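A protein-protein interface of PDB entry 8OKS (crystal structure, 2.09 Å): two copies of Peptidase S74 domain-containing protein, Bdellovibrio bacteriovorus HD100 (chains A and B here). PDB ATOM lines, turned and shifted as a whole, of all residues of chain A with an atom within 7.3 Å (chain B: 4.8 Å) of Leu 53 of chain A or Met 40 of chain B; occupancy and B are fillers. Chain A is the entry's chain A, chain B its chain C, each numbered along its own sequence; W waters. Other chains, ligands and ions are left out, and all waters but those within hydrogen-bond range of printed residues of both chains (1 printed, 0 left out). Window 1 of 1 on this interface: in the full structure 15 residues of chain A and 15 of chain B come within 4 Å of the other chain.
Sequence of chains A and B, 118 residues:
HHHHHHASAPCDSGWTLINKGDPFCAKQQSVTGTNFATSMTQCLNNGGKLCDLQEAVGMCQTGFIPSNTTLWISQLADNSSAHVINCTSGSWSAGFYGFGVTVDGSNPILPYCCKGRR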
ATOM      1  N   LYS A  20      12.150  11.431  23.961  1.00  0.00           N
ATOM      2  CA  LYS A  20      13.429  11.532  24.650  1.00  0.00           C
ATOM      3  C   LYS A  20      13.199  12.251  25.968  1.00  0.00           C
ATOM      4  O   LYS A  20      12.401  13.190  26.033  1.00  0.00           O
ATOM      5  CB  LYS A  20      14.474  12.273  23.807  1.00  0.00           C
ATOM      6  CG  LYS A  20      15.364  11.358  22.977  1.00  0.00           C
ATOM      7  CD  LYS A  20      16.475  10.750  23.819  1.00  0.00           C
ATOM      8  CE  LYS A  20      17.174   9.621  23.076  1.00  0.00           C
ATOM      9  NZ  LYS A  20      18.649   9.640  23.285  1.00  0.00           N
ATOM     10  N   GLY A  21      13.897  11.812  27.012  1.00  0.00           N
ATOM     11  CA  GLY A  21      13.602  12.343  28.333  1.00  0.00           C
ATOM     12  C   GLY A  21      12.173  12.020  28.714  1.00  0.00           C
ATOM     13  O   GLY A  21      11.664  10.931  28.426  1.00  0.00           O
ATOM     14  N   LEU A  50       9.716  28.365  23.221  1.00  0.00           N
ATOM     15  CA  LEU A  50      10.988  27.957  22.644  1.00  0.00           C
ATOM     16  C   LEU A  50      11.584  26.837  23.485  1.00  0.00           C
ATOM     17  O   LEU A  50      11.644  26.932  24.714  1.00  0.00           O
ATOM     18  CB  LEU A  50      11.956  29.139  22.569  1.00  0.00           C
ATOM     19  CG  LEU A  50      11.721  30.204  21.497  1.00  0.00           C
ATOM     20  CD1 LEU A  50      12.761  31.302  21.633  1.00  0.00           C
ATOM     21  CD2 LEU A  50      11.755  29.601  20.102  1.00  0.00           C
ATOM     22  N   CYS A  51      12.005  25.766  22.816  1.00  0.00           N
ATOM     23  CA  CYS A  51      12.530  24.594  23.502  1.00  0.00           C
ATOM     24  C   CYS A  51      13.810  24.945  24.252  1.00  0.00           C
ATOM     25  O   CYS A  51      14.598  25.787  23.817  1.00  0.00           O
ATOM     26  CB  CYS A  51      12.803  23.474  22.501  1.00  0.00           C
ATOM     27  SG  CYS A  51      11.421  23.096  21.395  1.00  0.00           S
ATOM     28  N   ASP A  52      14.029  24.272  25.380  1.00  0.00           N
ATOM     29  CA  ASP A  52      15.240  24.503  26.157  1.00  0.00           C
ATOM     30  C   ASP A  52      16.398  23.706  25.552  1.00  0.00           C
ATOM     31  O   ASP A  52      16.294  23.138  24.463  1.00  0.00           O
ATOM     32  CB  ASP A  52      15.002  24.167  27.629  1.00  0.00           C
ATOM     33  CG  ASP A  52      14.615  22.719  27.848  1.00  0.00           C
ATOM     34  OD1 ASP A  52      15.442  21.825  27.574  1.00  0.00           O
ATOM     35  OD2 ASP A  52      13.480  22.479  28.308  1.00  0.00           O
ATOM     36  N   LEU A  53      17.525  23.660  26.266  1.00  0.00           N
ATOM     37  CA  LEU A  53      18.717  22.993  25.748  1.00  0.00           C
ATOM     38  C   LEU A  53      18.498  21.491  25.602  1.00  0.00           C
ATOM     39  O   LEU A  53      18.804  20.903  24.555  1.00  0.00           O
ATOM     40  CB  LEU A  53      19.908  23.277  26.666  1.00  0.00           C
ATOM     41  CG  LEU A  53      21.106  22.330  26.579  1.00  0.00           C
ATOM     42  CD1 LEU A  53      21.824  22.514  25.254  1.00  0.00           C
ATOM     43  CD2 LEU A  53      22.058  22.553  27.747  1.00  0.00           C
ATOM     44  N   GLN A  54      17.968  20.850  26.647  1.00  0.00           N
ATOM     45  CA  GLN A  54      17.809  19.401  26.617  1.00  0.00           C
ATOM     46  C   GLN A  54      16.731  18.970  25.632  1.00  0.00           C
ATOM     47  O   GLN A  54      16.846  17.901  25.025  1.00  0.00           O
ATOM     48  CB  GLN A  54      17.500  18.879  28.018  1.00  0.00           C
ATOM     49  CG  GLN A  54      18.659  19.048  28.982  1.00  0.00           C
ATOM     50  CD  GLN A  54      18.375  18.468  30.349  1.00  0.00           C
ATOM     51  OE1 GLN A  54      18.792  17.353  30.659  1.00  0.00           O
ATOM     52  NE2 GLN A  54      17.665  19.225  31.177  1.00  0.00           N
ATOM     53  N   GLU A  55      15.691  19.783  25.447  1.00  0.00           N
ATOM     54  CA  GLU A  55      14.690  19.460  24.437  1.00  0.00           C
ATOM     55  C   GLU A  55      15.277  19.561  23.034  1.00  0.00           C
ATOM     56  O   GLU A  55      14.968  18.738  22.164  1.00  0.00           O
ATOM     57  CB  GLU A  55      13.473  20.369  24.598  1.00  0.00           C
ATOM     58  CG  GLU A  55      12.878  20.321  25.999  1.00  0.00           C
ATOM     59  CD  GLU A  55      11.629  21.166  26.147  1.00  0.00           C
ATOM     60  OE1 GLU A  55      11.688  22.376  25.846  1.00  0.00           O
ATOM     61  OE2 GLU A  55      10.589  20.618  26.572  1.00  0.00           O
ATOM     62  N   ALA A  56      16.145  20.549  22.801  1.00  0.00           N
ATOM     63  CA  ALA A  56      16.844  20.637  21.522  1.00  0.00           C
ATOM     64  C   ALA A  56      17.721  19.412  21.297  1.00  0.00           C
ATOM     65  O   ALA A  56      17.722  18.822  20.207  1.00  0.00           O
ATOM     66  CB  ALA A  56      17.677  21.917  21.466  1.00  0.00           C
ATOM     67  N   VAL A  57      18.468  19.009  22.329  1.00  0.00           N
ATOM     68  CA  VAL A  57      19.341  17.845  22.211  1.00  0.00           C
ATOM     69  C   VAL A  57      18.524  16.586  21.941  1.00  0.00           C
ATOM     70  O   VAL A  57      18.908  15.740  21.124  1.00  0.00           O
ATOM     71  CB  VAL A  57      20.207  17.705  23.477  1.00  0.00           C
ATOM     72  CG1 VAL A  57      20.933  16.369  23.492  1.00  0.00           C
ATOM     73  CG2 VAL A  57      21.193  18.861  23.570  1.00  0.00           C
ATOM     74  N   GLY A  58      17.377  16.451  22.610  1.00  0.00           N
ATOM     75  CA  GLY A  58      16.531  15.292  22.381  1.00  0.00           C
ATOM     76  C   GLY A  58      15.952  15.258  20.981  1.00  0.00           C
ATOM     77  O   GLY A  58      15.953  14.212  20.328  1.00  0.00           O
ATOM     78  N   MET A  59      15.450  16.399  20.499  1.00  0.00           N
ATOM     79  CA  MET A  59      14.939  16.459  19.132  1.00  0.00           C
ATOM     80  C   MET A  59      16.031  16.153  18.115  1.00  0.00           C
ATOM     81  O   MET A  59      15.752  15.558  17.067  1.00  0.00           O
ATOM     82  CB  MET A  59      14.331  17.832  18.852  1.00  0.00           C
ATOM     83  CG  MET A  59      13.119  18.180  19.690  1.00  0.00           C
ATOM     84  SD  MET A  59      12.490  19.818  19.280  1.00  0.00           S
ATOM     85  CE  MET A  59      13.858  20.868  19.737  1.00  0.00           C
ATOM     86  N   GLN A  61      18.654  14.132  18.716  1.00  0.00           N
ATOM     87  CA  GLN A  61      18.950  12.708  18.820  1.00  0.00           C
ATOM     88  C   GLN A  61      17.854  11.862  18.190  1.00  0.00           C
ATOM     89  O   GLN A  61      18.133  10.767  17.688  1.00  0.00           O
ATOM     90  CB  GLN A  61      19.150  12.319  20.285  1.00  0.00           C
ATOM     91  CG  GLN A  61      20.409  12.900  20.918  1.00  0.00           C
ATOM     92  CD  GLN A  61      20.583  12.487  22.368  1.00  0.00           C
ATOM     93  OE1 GLN A  61      19.744  11.784  22.931  1.00  0.00           O
ATOM     94  NE2 GLN A  61      21.677  12.927  22.981  1.00  0.00           N
ATOM     95  N   ILE A  73      17.502  28.296  21.389  1.00  0.00           N
ATOM     96  CA  ILE A  73      17.045  27.678  22.616  1.00  0.00           C
ATOM     97  C   ILE A  73      16.719  28.774  23.619  1.00  0.00           C
ATOM     98  O   ILE A  73      17.027  29.948  23.418  1.00  0.00           O
ATOM     99  CB  ILE A  73      18.066  26.656  23.181  1.00  0.00           C
ATOM    100  CG1 ILE A  73      19.402  27.325  23.506  1.00  0.00           C
ATOM    101  CG2 ILE A  73      18.231  25.492  22.218  1.00  0.00           C
ATOM    102  CD1 ILE A  73      20.284  26.495  24.423  1.00  0.00           C
ATOM    103  N   SER A  74      16.082  28.392  24.724  1.00  0.00           N
ATOM    104  CA  SER A  74      15.419  29.342  25.607  1.00  0.00           C
ATOM    105  C   SER A  74      16.365  30.080  26.547  1.00  0.00           C
ATOM    106  O   SER A  74      15.907  30.964  27.279  1.00  0.00           O
ATOM    107  CB  SER A  74      14.351  28.620  26.432  1.00  0.00           C
ATOM    108  OG  SER A  74      14.934  27.623  27.252  1.00  0.00           O
ATOM    109  N   GLN A  75      17.655  29.758  26.550  1.00  0.00           N
ATOM    110  CA  GLN A  75      18.577  30.336  27.519  1.00  0.00           C
ATOM    111  C   GLN A  75      19.213  31.612  26.985  1.00  0.00           C
ATOM    112  O   GLN A  75      19.509  31.726  25.791  1.00  0.00           O
ATOM    113  CB  GLN A  75      19.668  29.334  27.895  1.00  0.00           C
ATOM    114  CG  GLN A  75      20.460  29.737  29.130  1.00  0.00           C
ATOM    115  CD  GLN A  75      21.708  28.905  29.327  1.00  0.00           C
ATOM    116  OE1 GLN A  75      21.674  27.679  29.223  1.00  0.00           O
ATOM    117  NE2 GLN A  75      22.823  29.568  29.616  1.00  0.00           N
ATOM    118  N   VAL A  84      22.043  29.642  20.753  1.00  0.00           N
ATOM    119  CA  VAL A  84      21.564  28.781  19.685  1.00  0.00           C
ATOM    120  C   VAL A  84      22.174  27.401  19.874  1.00  0.00           C
ATOM    121  O   VAL A  84      23.258  27.236  20.445  1.00  0.00           O
ATOM    122  CB  VAL A  84      21.903  29.322  18.280  1.00  0.00           C
ATOM    123  CG1 VAL A  84      21.168  30.618  18.006  1.00  0.00           C
ATOM    124  CG2 VAL A  84      23.410  29.497  18.125  1.00  0.00           C
ATOM    125  N   ILE A  85      21.464  26.399  19.368  1.00  0.00           N
ATOM    126  CA  ILE A  85      21.966  25.036  19.285  1.00  0.00           C
ATOM    127  C   ILE A  85      21.992  24.633  17.819  1.00  0.00           C
ATOM    128  O   ILE A  85      20.996  24.804  17.104  1.00  0.00           O
ATOM    129  CB  ILE A  85      21.113  24.059  20.115  1.00  0.00           C
ATOM    130  CG1 ILE A  85      21.454  24.190  21.601  1.00  0.00           C
ATOM    131  CG2 ILE A  85      21.329  22.629  19.649  1.00  0.00           C
ATOM    132  CD1 ILE A  85      22.894  23.873  21.925  1.00  0.00           C
ATOM    133  N   TRP A  92      25.098  17.749  19.080  1.00  0.00           N
ATOM    134  CA  TRP A  92      24.723  19.140  19.276  1.00  0.00           C
ATOM    135  C   TRP A  92      25.946  19.980  19.624  1.00  0.00           C
ATOM    136  O   TRP A  92      26.922  19.488  20.196  1.00  0.00           O
ATOM    137  CB  TRP A  92      23.673  19.277  20.382  1.00  0.00           C
ATOM    138  CG  TRP A  92      24.165  18.843  21.730  1.00  0.00           C
ATOM    139  CD1 TRP A  92      24.178  17.573  22.228  1.00  0.00           C
ATOM    140  CD2 TRP A  92      24.717  19.681  22.753  1.00  0.00           C
ATOM    141  NE1 TRP A  92      24.703  17.567  23.497  1.00  0.00           N
ATOM    142  CE2 TRP A  92      25.042  18.848  23.843  1.00  0.00           C
ATOM    143  CE3 TRP A  92      24.968  21.053  22.853  1.00  0.00           C
ATOM    144  CZ2 TRP A  92      25.605  19.343  25.019  1.00  0.00           C
ATOM    145  CZ3 TRP A  92      25.527  21.542  24.021  1.00  0.00           C
ATOM    146  CH2 TRP A  92      25.839  20.689  25.088  1.00  0.00           C
ATOM    147  N   SER A  93      25.875  21.258  19.261  1.00  0.00           N
ATOM    148  CA  SER A  93      26.894  22.240  19.597  1.00  0.00           C
ATOM    149  C   SER A  93      26.200  23.550  19.938  1.00  0.00           C
ATOM    150  O   SER A  93      25.115  23.840  19.433  1.00  0.00           O
ATOM    151  CB  SER A  93      27.894  22.437  18.447  1.00  0.00           C
ATOM    152  OG  SER A  93      28.668  23.609  18.631  1.00  0.00           O
ATOM    153  N   ALA A  94      26.825  24.337  20.808  1.00  0.00           N
ATOM    154  CA  ALA A  94      26.210  25.547  21.331  1.00  0.00           C
ATOM    155  C   ALA A  94      26.899  26.791  20.784  1.00  0.00           C
ATOM    156  O   ALA A  94      28.107  26.796  20.529  1.00  0.00           O
ATOM    157  CB  ALA A  94      26.248  25.566  22.862  1.00  0.00           C
ATOM    158  N   PHE B  36      29.288  16.557  31.019  1.00  0.00           N
ATOM    159  CA  PHE B  36      27.967  17.161  30.863  1.00  0.00           C
ATOM    160  C   PHE B  36      27.154  16.468  29.777  1.00  0.00           C
ATOM    161  O   PHE B  36      25.981  16.131  29.984  1.00  0.00           O
ATOM    162  CB  PHE B  36      28.124  18.651  30.557  1.00  0.00           C
ATOM    163  CG  PHE B  36      26.824  19.396  30.452  1.00  0.00           C
ATOM    164  CD1 PHE B  36      25.979  19.502  31.544  1.00  0.00           C
ATOM    165  CD2 PHE B  36      26.453  20.000  29.263  1.00  0.00           C
ATOM    166  CE1 PHE B  36      24.786  20.193  31.449  1.00  0.00           C
ATOM    167  CE2 PHE B  36      25.262  20.694  29.162  1.00  0.00           C
ATOM    168  CZ  PHE B  36      24.427  20.790  30.256  1.00  0.00           C
ATOM    169  N   ALA B  37      27.756  16.263  28.602  1.00  0.00           N
ATOM    170  CA  ALA B  37      27.023  15.673  27.487  1.00  0.00           C
ATOM    171  C   ALA B  37      26.559  14.258  27.814  1.00  0.00           C
ATOM    172  O   ALA B  37      25.409  13.894  27.541  1.00  0.00           O
ATOM    173  CB  ALA B  37      27.890  15.678  26.229  1.00  0.00           C
ATOM    174  N   THR B  38      27.439  13.449  28.407  1.00  0.00           N
ATOM    175  CA  THR B  38      27.054  12.095  28.792  1.00  0.00           C
ATOM    176  C   THR B  38      25.999  12.112  29.893  1.00  0.00           C
ATOM    177  O   THR B  38      25.066  11.301  29.874  1.00  0.00           O
ATOM    178  CB  THR B  38      28.282  11.303  29.238  1.00  0.00           C
ATOM    179  OG1 THR B  38      29.302  11.395  28.235  1.00  0.00           O
ATOM    180  CG2 THR B  38      27.924   9.840  29.453  1.00  0.00           C
ATOM    181  N   SER B  39      26.131  13.025  30.858  1.00  0.00           N
ATOM    182  CA  SER B  39      25.105  13.179  31.884  1.00  0.00           C
ATOM    183  C   SER B  39      23.739  13.406  31.249  1.00  0.00           C
ATOM    184  O   SER B  39      22.767  12.695  31.550  1.00  0.00           O
ATOM    185  CB  SER B  39      25.467  14.341  32.813  1.00  0.00           C
ATOM    186  OG  SER B  39      26.576  14.026  33.638  1.00  0.00           O
ATOM    187  N   MET B  40      23.656  14.391  30.348  1.00  0.00           N
ATOM    188  CA  MET B  40      22.379  14.735  29.732  1.00  0.00           C
ATOM    189  C   MET B  40      21.844  13.592  28.878  1.00  0.00           C
ATOM    190  O   MET B  40      20.641  13.307  28.898  1.00  0.00           O
ATOM    191  CB  MET B  40      22.522  16.001  28.892  1.00  0.00           C
ATOM    192  CG  MET B  40      21.246  16.420  28.183  1.00  0.00           C
ATOM    193  SD  MET B  40      21.559  17.696  26.953  1.00  0.00           S
ATOM    194  CE  MET B  40      22.469  18.884  27.936  1.00  0.00           C
ATOM    195  N   THR B  41      22.717  12.928  28.117  1.00  0.00           N
ATOM    196  CA  THR B  41      22.264  11.830  27.268  1.00  0.00           C
ATOM    197  C   THR B  41      21.738  10.669  28.103  1.00  0.00           C
ATOM    198  O   THR B  41      20.728  10.048  27.750  1.00  0.00           O
ATOM    199  CB  THR B  41      23.397  11.365  26.354  1.00  0.00           C
ATOM    200  OG1 THR B  41      23.863  12.470  25.567  1.00  0.00           O
ATOM    201  CG2 THR B  41      22.915  10.262  25.425  1.00  0.00           C
ATOM    202  N   GLN B  42      22.401  10.363  29.221  1.00  0.00           N
ATOM    203  CA  GLN B  42      21.937   9.272  30.070  1.00  0.00           C
ATOM    204  C   GLN B  42      20.606   9.617  30.723  1.00  0.00           C
ATOM    205  O   GLN B  42      19.714   8.764  30.820  1.00  0.00           O
ATOM    206  CB  GLN B  42      22.993   8.941  31.123  1.00  0.00           C
ATOM    207  CG  GLN B  42      24.198   8.194  30.565  1.00  0.00           C
ATOM    208  CD  GLN B  42      25.224   7.862  31.628  1.00  0.00           C
ATOM    209  OE1 GLN B  42      25.010   8.119  32.812  1.00  0.00           O
ATOM    210  NE2 GLN B  42      26.347   7.287  31.211  1.00  0.00           N
ATOM    211  N   CYS B  43      20.446  10.868  31.156  1.00  0.00           N
ATOM    212  CA  CYS B  43      19.163  11.284  31.710  1.00  0.00           C
ATOM    213  C   CYS B  43      18.058  11.182  30.660  1.00  0.00           C
ATOM    214  O   CYS B  43      16.978  10.646  30.931  1.00  0.00           O
ATOM    215  CB  CYS B  43      19.261  12.709  32.253  1.00  0.00           C
ATOM    216  SG  CYS B  43      20.134  12.865  33.836  1.00  0.00           S
ATOM    217  N   LEU B  44      18.316  11.685  29.446  1.00  0.00           N
ATOM    218  CA  LEU B  44      17.332  11.614  28.370  1.00  0.00           C
ATOM    219  C   LEU B  44      17.004  10.176  28.002  1.00  0.00           C
ATOM    220  O   LEU B  44      15.878   9.887  27.591  1.00  0.00           O
ATOM    221  CB  LEU B  44      17.848  12.369  27.142  1.00  0.00           C
ATOM    222  CG  LEU B  44      17.883  13.895  27.198  1.00  0.00           C
ATOM    223  CD1 LEU B  44      18.573  14.451  25.963  1.00  0.00           C
ATOM    224  CD2 LEU B  44      16.477  14.451  27.328  1.00  0.00           C
ATOM    225  N   LEU B  50      18.283  16.462  32.953  1.00  0.00           N
ATOM    226  CA  LEU B  50      19.082  17.032  34.028  1.00  0.00           C
ATOM    227  C   LEU B  50      18.244  18.001  34.852  1.00  0.00           C
ATOM    228  O   LEU B  50      17.488  18.813  34.312  1.00  0.00           O
ATOM    229  CB  LEU B  50      20.306  17.750  33.459  1.00  0.00           C
ATOM    230  CG  LEU B  50      21.452  16.871  32.958  1.00  0.00           C
ATOM    231  CD1 LEU B  50      22.392  17.691  32.095  1.00  0.00           C
ATOM    232  CD2 LEU B  50      22.198  16.243  34.122  1.00  0.00           C
ATOM    233  N   SER B  74      21.063  22.107  34.360  1.00  0.00           N
ATOM    234  CA  SER B  74      20.697  22.149  32.952  1.00  0.00           C
ATOM    235  C   SER B  74      20.936  23.509  32.301  1.00  0.00           C
ATOM    236  O   SER B  74      20.360  23.784  31.242  1.00  0.00           O
ATOM    237  CB  SER B  74      19.232  21.741  32.782  1.00  0.00           C
ATOM    238  OG  SER B  74      18.367  22.646  33.445  1.00  0.00           O
ATOM    239  N   LEU B  76      23.651  26.245  30.621  1.00  0.00           N
ATOM    240  CA  LEU B  76      24.975  26.532  30.094  1.00  0.00           C
ATOM    241  C   LEU B  76      25.563  27.764  30.772  1.00  0.00           C
ATOM    242  O   LEU B  76      24.845  28.686  31.169  1.00  0.00           O
ATOM    243  CB  LEU B  76      24.913  26.761  28.582  1.00  0.00           C
ATOM    244  CG  LEU B  76      24.350  25.652  27.691  1.00  0.00           C
ATOM    245  CD1 LEU B  76      24.254  26.126  26.248  1.00  0.00           C
ATOM    246  CD2 LEU B  76      25.211  24.406  27.791  1.00  0.00           C
HETATM  247  O   HOH W   1      25.644  31.166  28.885  1.00  0.00           O
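The side-chain hydroxyl of Thr 41 of chain B is in hydrogen-bond range of the side-chain amide nitrogen of Gln 61 of chain A, 3.4 Å away. N of Gly 21 of chain A is in hydrogen-bond range of O of Leu 44 of chain B (2.8 Å). The backbone NH of Leu 50 of chain B lies within hydrogen-bond range of the side-chain amide oxygen of Gln 54 of chain A (2.5 Å). The backbone carbonyl oxygen (O) of Leu 76 of chain B lies within hydrogen-bond range of the side-chain amide nitrogen (NE2) of Gln 75 of chain A, 2.7 Å away.
O of Ala 37 of chain B sits at hydrogen-bond distance from OG1 of Thr 41 of chain B, 2.9 Å away. The side-chain amide oxygen of Gln 61 of chain A lies within hydrogen-bond range of the side-chain amino group of Lys 20 of chain A. OD1 of Asp 52 of chain A sits at hydrogen-bond distance from N of Gln 54 of chain A (2.9 Å).
Leu 44 of chain B touches Lys 20 of chain A. Leu 53 of chain A touches Phe 36 of chain B. Leu 53 of chain A touches Met 40 of chain B. Leu 53 of chain A touches Leu 76 of chain B (CD2 to CD2, 3.7 Å). CG of Met 40 of chain B touches OE1 of Gln 54 of chain A (3.6 Å). CD1 of Leu 44 of chain B touches O of Gln 54 of chain A, 3.97 Å away. NE2 of Gln 54 of chain A touches CB of Ser 74 of chain B, at 3.4 Å. Met 40 of chain B touches Val 57 of chain A (SD to CG2, 3.6 Å). Val 57 of chain A touches Leu 44 of chain B. Leu 76 of chain B touches Ala 94 of chain A.
Leu 53 of chain A touches just these residues of chain B: Phe 36 (3.9 Å), Met 40 (3.7 Å) and Leu 76 (3.7 Å). Met 40 of chain B touches just these residues of chain A: Leu 53, Gln 54 and Val 57. Printed residues of chain A within 4 Å of Leu 50 of chain B: Gln 54 (2.5 Å). Of the printed residues of chain B, Ala 94 of chain A touches Leu 76 (3.97 Å). Of the printed residues of chain A, Leu 76 of chain B touches Leu 53 (3.7 Å), Gln 75 (2.7 Å) and Ala 94 (3.97 Å). Of the printed residues of chain B, Gln 61 of chain A touches Thr 41 (3.4 Å). Of the printed residues of chain B, Val 57 of chain A touches Met 40 (3.6 Å) and Leu 44 (3.9 Å). The nearest residue of chain B that does not touch Leu 53 of chain A is Ser 74 of chain B (4.1 Å).
Hydrophobic or aromatic side chains of chain A within 4 Å of the printed part of chain B: Leu 53, Val 57 and Ala 94. Hydrophobic or aromatic side chains of chain B within 4 Å of the printed part of chain A: Phe 36, Met 40, Leu 44, Leu 50 and Leu 76.
Positions printed for both chains: 50 and 74. Of the 14 pairs that touch across the chains among the printed residues, none has its exchanged pair printed and touching as well.
Water W1 lies within hydrogen-bond range of the side-chain amide nitrogen (NE2) of Gln 75 of chain A (3.3 Å) and the backbone carbonyl oxygen (O) of Leu 76 of chain B (3.5 Å).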
